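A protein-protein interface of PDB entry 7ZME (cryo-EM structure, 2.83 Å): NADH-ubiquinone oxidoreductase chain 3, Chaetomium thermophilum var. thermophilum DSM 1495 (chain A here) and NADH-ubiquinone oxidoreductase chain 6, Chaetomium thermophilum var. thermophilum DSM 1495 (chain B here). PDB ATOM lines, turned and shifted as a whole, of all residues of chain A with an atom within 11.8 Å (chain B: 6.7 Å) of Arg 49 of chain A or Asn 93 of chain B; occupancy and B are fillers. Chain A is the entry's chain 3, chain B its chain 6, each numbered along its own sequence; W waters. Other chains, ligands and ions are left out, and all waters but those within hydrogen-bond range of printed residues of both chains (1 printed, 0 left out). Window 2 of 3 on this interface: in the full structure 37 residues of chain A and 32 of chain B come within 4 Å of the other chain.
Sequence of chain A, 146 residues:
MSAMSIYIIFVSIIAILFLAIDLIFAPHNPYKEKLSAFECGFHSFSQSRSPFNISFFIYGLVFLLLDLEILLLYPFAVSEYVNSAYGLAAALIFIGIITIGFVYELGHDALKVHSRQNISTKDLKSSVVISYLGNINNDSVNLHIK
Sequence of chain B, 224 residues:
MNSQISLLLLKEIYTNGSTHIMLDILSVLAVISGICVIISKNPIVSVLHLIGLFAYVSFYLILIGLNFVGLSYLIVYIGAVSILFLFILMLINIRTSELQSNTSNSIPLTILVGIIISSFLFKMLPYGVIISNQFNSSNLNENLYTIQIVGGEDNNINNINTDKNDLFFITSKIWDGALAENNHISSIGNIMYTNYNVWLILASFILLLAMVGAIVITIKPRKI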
ATOM      1  N   ALA A  37     -15.637  21.371   3.296  1.00  0.00           N
ATOM      2  CA  ALA A  37     -14.887  22.511   2.730  1.00  0.00           C
ATOM      3  C   ALA A  37     -15.351  23.805   3.369  1.00  0.00           C
ATOM      4  O   ALA A  37     -16.563  23.944   3.556  1.00  0.00           O
ATOM      5  CB  ALA A  37     -15.090  22.571   1.240  1.00  0.00           C
ATOM      6  N   GLU A  39     -16.483  27.563   3.301  1.00  0.00           N
ATOM      7  CA  GLU A  39     -17.127  28.432   2.288  1.00  0.00           C
ATOM      8  C   GLU A  39     -17.794  29.523   3.110  1.00  0.00           C
ATOM      9  O   GLU A  39     -18.950  29.874   2.815  1.00  0.00           O
ATOM     10  CB  GLU A  39     -17.983  27.611   1.316  1.00  0.00           C
ATOM     11  CG  GLU A  39     -18.645  28.392   0.188  1.00  0.00           C
ATOM     12  CD  GLU A  39     -17.790  29.222  -0.757  1.00  0.00           C
ATOM     13  OE1 GLU A  39     -17.119  30.158  -0.291  1.00  0.00           O
ATOM     14  OE2 GLU A  39     -17.834  28.952  -1.964  1.00  0.00           O
ATOM     15  N   SER A  44     -21.711  25.305  -0.757  1.00  0.00           N
ATOM     16  CA  SER A  44     -21.952  25.801  -2.100  1.00  0.00           C
ATOM     17  C   SER A  44     -21.604  24.708  -3.097  1.00  0.00           C
ATOM     18  O   SER A  44     -21.284  23.576  -2.727  1.00  0.00           O
ATOM     19  CB  SER A  44     -21.146  27.077  -2.369  1.00  0.00           C
ATOM     20  OG  SER A  44     -21.585  27.725  -3.548  1.00  0.00           O
ATOM     21  N   PHE A  45     -21.676  25.059  -4.377  1.00  0.00           N
ATOM     22  CA  PHE A  45     -21.291  24.143  -5.438  1.00  0.00           C
ATOM     23  C   PHE A  45     -19.786  23.926  -5.420  1.00  0.00           C
ATOM     24  O   PHE A  45     -19.013  24.887  -5.371  1.00  0.00           O
ATOM     25  CB  PHE A  45     -21.724  24.692  -6.796  1.00  0.00           C
ATOM     26  CG  PHE A  45     -23.113  25.257  -6.812  1.00  0.00           C
ATOM     27  CD1 PHE A  45     -23.340  26.585  -6.510  1.00  0.00           C
ATOM     28  CD2 PHE A  45     -24.193  24.456  -7.133  1.00  0.00           C
ATOM     29  CE1 PHE A  45     -24.615  27.104  -6.524  1.00  0.00           C
ATOM     30  CE2 PHE A  45     -25.469  24.970  -7.149  1.00  0.00           C
ATOM     31  CZ  PHE A  45     -25.680  26.297  -6.844  1.00  0.00           C
ATOM     32  N   SER A  46     -19.369  22.666  -5.459  1.00  0.00           N
ATOM     33  CA  SER A  46     -17.955  22.351  -5.600  1.00  0.00           C
ATOM     34  C   SER A  46     -17.542  22.536  -7.053  1.00  0.00           C
ATOM     35  O   SER A  46     -17.946  21.760  -7.925  1.00  0.00           O
ATOM     36  CB  SER A  46     -17.683  20.923  -5.136  1.00  0.00           C
ATOM     37  OG  SER A  46     -16.307  20.600  -5.240  1.00  0.00           O
ATOM     38  N   GLN A  47     -16.744  23.574  -7.320  1.00  0.00           N
ATOM     39  CA  GLN A  47     -16.360  23.893  -8.688  1.00  0.00           C
ATOM     40  C   GLN A  47     -14.855  24.038  -8.867  1.00  0.00           C
ATOM     41  O   GLN A  47     -14.420  24.512  -9.921  1.00  0.00           O
ATOM     42  CB  GLN A  47     -17.043  25.183  -9.156  1.00  0.00           C
ATOM     43  CG  GLN A  47     -18.521  25.274  -8.826  1.00  0.00           C
ATOM     44  CD  GLN A  47     -19.047  26.689  -8.913  1.00  0.00           C
ATOM     45  OE1 GLN A  47     -18.693  27.543  -8.107  1.00  0.00           O
ATOM     46  NE2 GLN A  47     -19.896  26.943  -9.899  1.00  0.00           N
ATOM     47  N   SER A  48     -14.047  23.647  -7.886  1.00  0.00           N
ATOM     48  CA  SER A  48     -12.609  23.849  -7.974  1.00  0.00           C
ATOM     49  C   SER A  48     -11.911  22.796  -8.823  1.00  0.00           C
ATOM     50  O   SER A  48     -10.704  22.910  -9.052  1.00  0.00           O
ATOM     51  CB  SER A  48     -12.001  23.871  -6.570  1.00  0.00           C
ATOM     52  OG  SER A  48     -12.368  25.052  -5.886  1.00  0.00           O
ATOM     53  N   ARG A  49     -12.631  21.778  -9.284  1.00  0.00           N
ATOM     54  CA  ARG A  49     -12.075  20.743 -10.144  1.00  0.00           C
ATOM     55  C   ARG A  49     -12.702  20.791 -11.532  1.00  0.00           C
ATOM     56  O   ARG A  49     -12.817  19.770 -12.208  1.00  0.00           O
ATOM     57  CB  ARG A  49     -12.252  19.363  -9.516  1.00  0.00           C
ATOM     58  CG  ARG A  49     -11.530  19.199  -8.194  1.00  0.00           C
ATOM     59  CD  ARG A  49     -10.039  19.369  -8.370  1.00  0.00           C
ATOM     60  NE  ARG A  49      -9.291  18.914  -7.205  1.00  0.00           N
ATOM     61  CZ  ARG A  49      -8.701  19.720  -6.331  1.00  0.00           C
ATOM     62  NH1 ARG A  49      -8.770  21.034  -6.483  1.00  0.00           N
ATOM     63  NH2 ARG A  49      -8.041  19.211  -5.303  1.00  0.00           N
ATOM     64  N   SER A  50     -13.111  21.981 -11.957  1.00  0.00           N
ATOM     65  CA  SER A  50     -13.705  22.270 -13.249  1.00  0.00           C
ATOM     66  C   SER A  50     -12.915  23.387 -13.910  1.00  0.00           C
ATOM     67  O   SER A  50     -12.304  24.203 -13.215  1.00  0.00           O
ATOM     68  CB  SER A  50     -15.176  22.690 -13.102  1.00  0.00           C
ATOM     69  OG  SER A  50     -15.963  21.638 -12.578  1.00  0.00           O
ATOM     70  N   PRO A  51     -12.900  23.446 -15.241  1.00  0.00           N
ATOM     71  CA  PRO A  51     -12.043  24.426 -15.925  1.00  0.00           C
ATOM     72  C   PRO A  51     -12.355  25.850 -15.488  1.00  0.00           C
ATOM     73  O   PRO A  51     -13.509  26.281 -15.483  1.00  0.00           O
ATOM     74  CB  PRO A  51     -12.358  24.200 -17.406  1.00  0.00           C
ATOM     75  CG  PRO A  51     -12.872  22.810 -17.476  1.00  0.00           C
ATOM     76  CD  PRO A  51     -13.610  22.578 -16.196  1.00  0.00           C
ATOM     77  N   PHE A  52     -11.305  26.579 -15.125  1.00  0.00           N
ATOM     78  CA  PHE A  52     -11.405  27.914 -14.559  1.00  0.00           C
ATOM     79  C   PHE A  52     -10.676  28.899 -15.460  1.00  0.00           C
ATOM     80  O   PHE A  52      -9.679  28.557 -16.098  1.00  0.00           O
ATOM     81  CB  PHE A  52     -10.818  27.945 -13.140  1.00  0.00           C
ATOM     82  CG  PHE A  52     -10.982  29.260 -12.433  1.00  0.00           C
ATOM     83  CD1 PHE A  52     -12.121  29.523 -11.694  1.00  0.00           C
ATOM     84  CD2 PHE A  52      -9.984  30.217 -12.477  1.00  0.00           C
ATOM     85  CE1 PHE A  52     -12.271  30.725 -11.037  1.00  0.00           C
ATOM     86  CE2 PHE A  52     -10.129  31.417 -11.820  1.00  0.00           C
ATOM     87  CZ  PHE A  52     -11.271  31.673 -11.100  1.00  0.00           C
ATOM     88  N   ASN A  53     -11.174  30.127 -15.506  1.00  0.00           N
ATOM     89  CA  ASN A  53     -10.630  31.138 -16.400  1.00  0.00           C
ATOM     90  C   ASN A  53      -9.440  31.828 -15.746  1.00  0.00           C
ATOM     91  O   ASN A  53      -9.586  32.483 -14.709  1.00  0.00           O
ATOM     92  CB  ASN A  53     -11.697  32.164 -16.773  1.00  0.00           C
ATOM     93  CG  ASN A  53     -11.146  33.284 -17.621  1.00  0.00           C
ATOM     94  OD1 ASN A  53     -10.626  33.051 -18.710  1.00  0.00           O
ATOM     95  ND2 ASN A  53     -11.250  34.510 -17.125  1.00  0.00           N
ATOM     96  N   ILE A  54      -8.269  31.686 -16.355  1.00  0.00           N
ATOM     97  CA  ILE A  54      -7.092  32.457 -15.982  1.00  0.00           C
ATOM     98  C   ILE A  54      -6.912  33.559 -17.012  1.00  0.00           C
ATOM     99  O   ILE A  54      -6.674  33.289 -18.195  1.00  0.00           O
ATOM    100  CB  ILE A  54      -5.835  31.578 -15.872  1.00  0.00           C
ATOM    101  CG1 ILE A  54      -5.965  30.584 -14.712  1.00  0.00           C
ATOM    102  CG2 ILE A  54      -4.591  32.439 -15.707  1.00  0.00           C
ATOM    103  CD1 ILE A  54      -6.592  29.273 -15.063  1.00  0.00           C
ATOM    104  N   ASN B  42      -5.234  11.415 -12.580  1.00  0.00           N
ATOM    105  CA  ASN B  42      -5.355  12.875 -12.336  1.00  0.00           C
ATOM    106  C   ASN B  42      -4.255  13.617 -13.105  1.00  0.00           C
ATOM    107  O   ASN B  42      -3.080  13.253 -12.947  1.00  0.00           O
ATOM    108  CB  ASN B  42      -5.386  13.203 -10.842  1.00  0.00           C
ATOM    109  CG  ASN B  42      -5.589  14.672 -10.552  1.00  0.00           C
ATOM    110  OD1 ASN B  42      -4.775  15.299  -9.886  1.00  0.00           O
ATOM    111  ND2 ASN B  42      -6.673  15.230 -11.052  1.00  0.00           N
ATOM    112  N   PRO B  43      -4.594  14.637 -13.926  1.00  0.00           N
ATOM    113  CA  PRO B  43      -3.598  15.425 -14.654  1.00  0.00           C
ATOM    114  C   PRO B  43      -2.616  16.168 -13.740  1.00  0.00           C
ATOM    115  O   PRO B  43      -1.477  16.285 -14.107  1.00  0.00           O
ATOM    116  CB  PRO B  43      -4.465  16.402 -15.452  1.00  0.00           C
ATOM    117  CG  PRO B  43      -5.771  15.681 -15.611  1.00  0.00           C
ATOM    118  CD  PRO B  43      -5.962  15.021 -14.266  1.00  0.00           C
ATOM    119  N   ILE B  88      -3.560  23.288 -17.206  1.00  0.00           N
ATOM    120  CA  ILE B  88      -4.410  22.100 -16.886  1.00  0.00           C
ATOM    121  C   ILE B  88      -5.643  22.554 -16.105  1.00  0.00           C
ATOM    122  O   ILE B  88      -6.690  21.906 -16.212  1.00  0.00           O
ATOM    123  CB  ILE B  88      -3.584  21.053 -16.116  1.00  0.00           C
ATOM    124  CG1 ILE B  88      -2.477  20.450 -16.982  1.00  0.00           C
ATOM    125  CG2 ILE B  88      -4.468  19.974 -15.513  1.00  0.00           C
ATOM    126  CD1 ILE B  88      -1.474  19.643 -16.203  1.00  0.00           C
ATOM    127  N   LEU B  89      -5.533  23.668 -15.390  1.00  0.00           N
ATOM    128  CA  LEU B  89      -6.634  24.163 -14.535  1.00  0.00           C
ATOM    129  C   LEU B  89      -7.534  25.060 -15.376  1.00  0.00           C
ATOM    130  O   LEU B  89      -8.647  25.349 -14.930  1.00  0.00           O
ATOM    131  CB  LEU B  89      -6.020  24.948 -13.374  1.00  0.00           C
ATOM    132  CG  LEU B  89      -5.308  24.125 -12.311  1.00  0.00           C
ATOM    133  CD1 LEU B  89      -5.296  24.894 -11.004  1.00  0.00           C
ATOM    134  CD2 LEU B  89      -5.997  22.784 -12.139  1.00  0.00           C
ATOM    135  N   MET B  90      -7.076  25.449 -16.562  1.00  0.00           N
ATOM    136  CA  MET B  90      -7.867  26.283 -17.455  1.00  0.00           C
ATOM    137  C   MET B  90      -8.520  25.501 -18.587  1.00  0.00           C
ATOM    138  O   MET B  90      -9.633  25.843 -18.997  1.00  0.00           O
ATOM    139  CB  MET B  90      -6.979  27.401 -18.011  1.00  0.00           C
ATOM    140  CG  MET B  90      -7.661  28.393 -18.922  1.00  0.00           C
ATOM    141  SD  MET B  90      -6.500  29.660 -19.464  1.00  0.00           S
ATOM    142  CE  MET B  90      -5.470  28.739 -20.593  1.00  0.00           C
ATOM    143  N   LEU B  91      -7.877  24.425 -19.051  1.00  0.00           N
ATOM    144  CA  LEU B  91      -8.387  23.718 -20.255  1.00  0.00           C
ATOM    145  C   LEU B  91      -8.828  22.279 -19.957  1.00  0.00           C
ATOM    146  O   LEU B  91      -9.244  21.608 -20.909  1.00  0.00           O
ATOM    147  CB  LEU B  91      -7.298  23.728 -21.335  1.00  0.00           C
ATOM    148  CG  LEU B  91      -6.545  25.038 -21.553  1.00  0.00           C
ATOM    149  CD1 LEU B  91      -5.300  24.808 -22.392  1.00  0.00           C
ATOM    150  CD2 LEU B  91      -7.433  26.081 -22.203  1.00  0.00           C
ATOM    151  N   ILE B  92      -8.707  21.792 -18.721  1.00  0.00           N
ATOM    152  CA  ILE B  92      -9.062  20.360 -18.484  1.00  0.00           C
ATOM    153  C   ILE B  92     -10.066  20.223 -17.346  1.00  0.00           C
ATOM    154  O   ILE B  92      -9.820  20.824 -16.290  1.00  0.00           O
ATOM    155  CB  ILE B  92      -7.808  19.493 -18.216  1.00  0.00           C
ATOM    156  CG1 ILE B  92      -6.758  19.609 -19.322  1.00  0.00           C
ATOM    157  CG2 ILE B  92      -8.180  18.044 -17.940  1.00  0.00           C
ATOM    158  CD1 ILE B  92      -5.518  18.789 -19.070  1.00  0.00           C
ATOM    159  N   ASN B  93     -11.194  19.547 -17.578  1.00  0.00           N
ATOM    160  CA  ASN B  93     -12.100  19.211 -16.446  1.00  0.00           C
ATOM    161  C   ASN B  93     -11.406  18.124 -15.612  1.00  0.00           C
ATOM    162  O   ASN B  93     -11.368  16.980 -16.081  1.00  0.00           O
ATOM    163  CB  ASN B  93     -13.523  18.864 -16.892  1.00  0.00           C
ATOM    164  CG  ASN B  93     -14.553  18.963 -15.787  1.00  0.00           C
ATOM    165  OD1 ASN B  93     -14.261  18.714 -14.621  1.00  0.00           O
ATOM    166  ND2 ASN B  93     -15.775  19.309 -16.150  1.00  0.00           N
ATOM    167  N   ILE B  94     -10.885  18.467 -14.433  1.00  0.00           N
ATOM    168  CA  ILE B  94     -10.141  17.513 -13.615  1.00  0.00           C
ATOM    169  C   ILE B  94     -11.016  16.328 -13.231  1.00  0.00           C
ATOM    170  O   ILE B  94     -10.576  15.174 -13.276  1.00  0.00           O
ATOM    171  CB  ILE B  94      -9.564  18.214 -12.370  1.00  0.00           C
ATOM    172  CG1 ILE B  94      -8.408  19.135 -12.758  1.00  0.00           C
ATOM    173  CG2 ILE B  94      -9.097  17.193 -11.345  1.00  0.00           C
ATOM    174  CD1 ILE B  94      -7.152  18.401 -13.128  1.00  0.00           C
ATOM    175  N   ARG B  95     -12.265  16.592 -12.849  1.00  0.00           N
ATOM    176  CA  ARG B  95     -13.115  15.530 -12.319  1.00  0.00           C
ATOM    177  C   ARG B  95     -13.495  14.533 -13.406  1.00  0.00           C
ATOM    178  O   ARG B  95     -13.496  13.320 -13.172  1.00  0.00           O
ATOM    179  CB  ARG B  95     -14.354  16.138 -11.659  1.00  0.00           C
ATOM    180  CG  ARG B  95     -15.237  15.154 -10.894  1.00  0.00           C
ATOM    181  CD  ARG B  95     -16.316  14.550 -11.777  1.00  0.00           C
ATOM    182  NE  ARG B  95     -17.215  15.570 -12.306  1.00  0.00           N
ATOM    183  CZ  ARG B  95     -18.039  15.380 -13.330  1.00  0.00           C
ATOM    184  NH1 ARG B  95     -18.076  14.205 -13.942  1.00  0.00           N
ATOM    185  NH2 ARG B  95     -18.823  16.365 -13.745  1.00  0.00           N
ATOM    186  N   THR B  96     -13.760  15.036 -14.614  1.00  0.00           N
ATOM    187  CA  THR B  96     -14.160  14.139 -15.732  1.00  0.00           C
ATOM    188  C   THR B  96     -12.945  13.368 -16.252  1.00  0.00           C
ATOM    189  O   THR B  96     -13.139  12.236 -16.693  1.00  0.00           O
ATOM    190  CB  THR B  96     -14.866  14.909 -16.851  1.00  0.00           C
ATOM    191  OG1 THR B  96     -13.898  15.688 -17.551  1.00  0.00           O
ATOM    192  CG2 THR B  96     -15.999  15.780 -16.355  1.00  0.00           C
ATOM    193  N   SER B  97     -11.752  13.956 -16.214  1.00  0.00           N
ATOM    194  CA  SER B  97     -10.503  13.259 -16.615  1.00  0.00           C
ATOM    195  C   SER B  97     -10.182  12.101 -15.666  1.00  0.00           C
ATOM    196  O   SER B  97      -9.720  11.064 -16.152  1.00  0.00           O
ATOM    197  CB  SER B  97      -9.353  14.230 -16.708  1.00  0.00           C
ATOM    198  OG  SER B  97      -9.032  14.760 -15.436  1.00  0.00           O
ATOM    199  N   GLU B  98     -10.362  12.290 -14.359  1.00  0.00           N
ATOM    200  CA  GLU B  98     -10.134  11.194 -13.374  1.00  0.00           C
ATOM    201  C   GLU B  98     -11.133  10.073 -13.655  1.00  0.00           C
ATOM    202  O   GLU B  98     -10.757   8.901 -13.510  1.00  0.00           O
ATOM    203  CB  GLU B  98     -10.296  11.682 -11.934  1.00  0.00           C
ATOM    204  CG  GLU B  98      -9.206  12.626 -11.472  1.00  0.00           C
ATOM    205  CD  GLU B  98      -9.502  13.253 -10.122  1.00  0.00           C
ATOM    206  OE1 GLU B  98     -10.689  13.517  -9.846  1.00  0.00           O
ATOM    207  OE2 GLU B  98      -8.550  13.463  -9.345  1.00  0.00           O
HETATM  208  O   HOH W   1      -9.466  23.818 -12.354  1.00  0.00           O
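The backbone carbonyl oxygen (O) of Arg 49 of chain A lies close to the side-chain amide oxygen (OD1) of Asn 93 of chain B (3.0 Å).
O of Arg 49 of chain A is in hydrogen-bond range of N of Ile 94 of chain B.
The backbone NH of Arg 95 of chain B lies within hydrogen-bond range of the backbone carbonyl oxygen of Arg 49 of chain A (3.3 Å).
The backbone NH (N) of Phe 52 of chain A lies within hydrogen-bond range of the backbone carbonyl oxygen (O) of Leu 89 of chain B (2.9 Å).
The backbone NH of Arg 95 of chain B sits close to the side-chain amide oxygen of Asn 93 of chain B (3.4 Å).
The backbone carbonyl oxygen (O) of Asn 93 of chain B is in hydrogen-bond range of the side-chain hydroxyl (OG1) of Thr 96 of chain B, 3.2 Å away.
The backbone carbonyl oxygen of Asn 93 of chain B sits at hydrogen-bond distance from the side-chain hydroxyl of Ser 97 of chain B (3.3 Å).
O of Ile 94 of chain B lies within hydrogen-bond range of OG of Ser 97 of chain B.
OD1 of Asn 93 of chain B touches CA of Ser 50 of chain A, at 3.9 Å.
Pro 51 of chain A touches Leu 89 of chain B (CA to O, 3.7 Å).
O of Met 90 of chain B touches CB of Pro 51 of chain A, at 3.6 Å.
Pro 51 of chain A touches Ile 92 of chain B (CG to C, 3.8 Å).
N of Asn 93 of chain B touches CG of Pro 51 of chain A (3.7 Å).
Phe 52 of chain A touches Met 90 of chain B (O to CA, 3.2 Å).
CD1 of Ile 54 of chain A touches CB of Met 90 of chain B, at 3.5 Å.
Of the printed residues of chain A, Asn 93 of chain B touches Arg 49 (3.0 Å), Ser 50 (3.9 Å) and Pro 51 (3.7 Å).
Of chain A, only Arg 49 comes within 4 Å of Arg 95 of chain B.
Thr 96 of chain B touches none of the printed residues of chain A.
Printed residues of chain B within 4 Å of Phe 52 of chain A: Leu 89 (2.9 Å) and Met 90 (3.2 Å).
Printed residues of chain B within 4 Å of Ile 54 of chain A: Met 90.
Of the printed residues of chain B, Pro 51 of chain A touches Leu 89, Met 90, Ile 92 and Asn 93.
The nearest printed residue of chain B that does not touch Ile 54 of chain A is Leu 89 of chain B (4.3 Å).
Hydrophobic or aromatic side chains of chain B within 4 Å of the printed part of chain A: Met 90 and Ile 94.
Hydrophobic or aromatic side chains of chain A that line the printed part of chain B: Pro 51, Phe 52 and Ile 54.
Among the printed residues, 11 pairs touch across the chains.
Among the printed residues, no Asp or Glu carboxylate lies within 4 Å of a Lys or Arg side-chain nitrogen of the other chain.
Water W1 bridges O of Ser 50 of chain A and O of Leu 89 of chain B.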
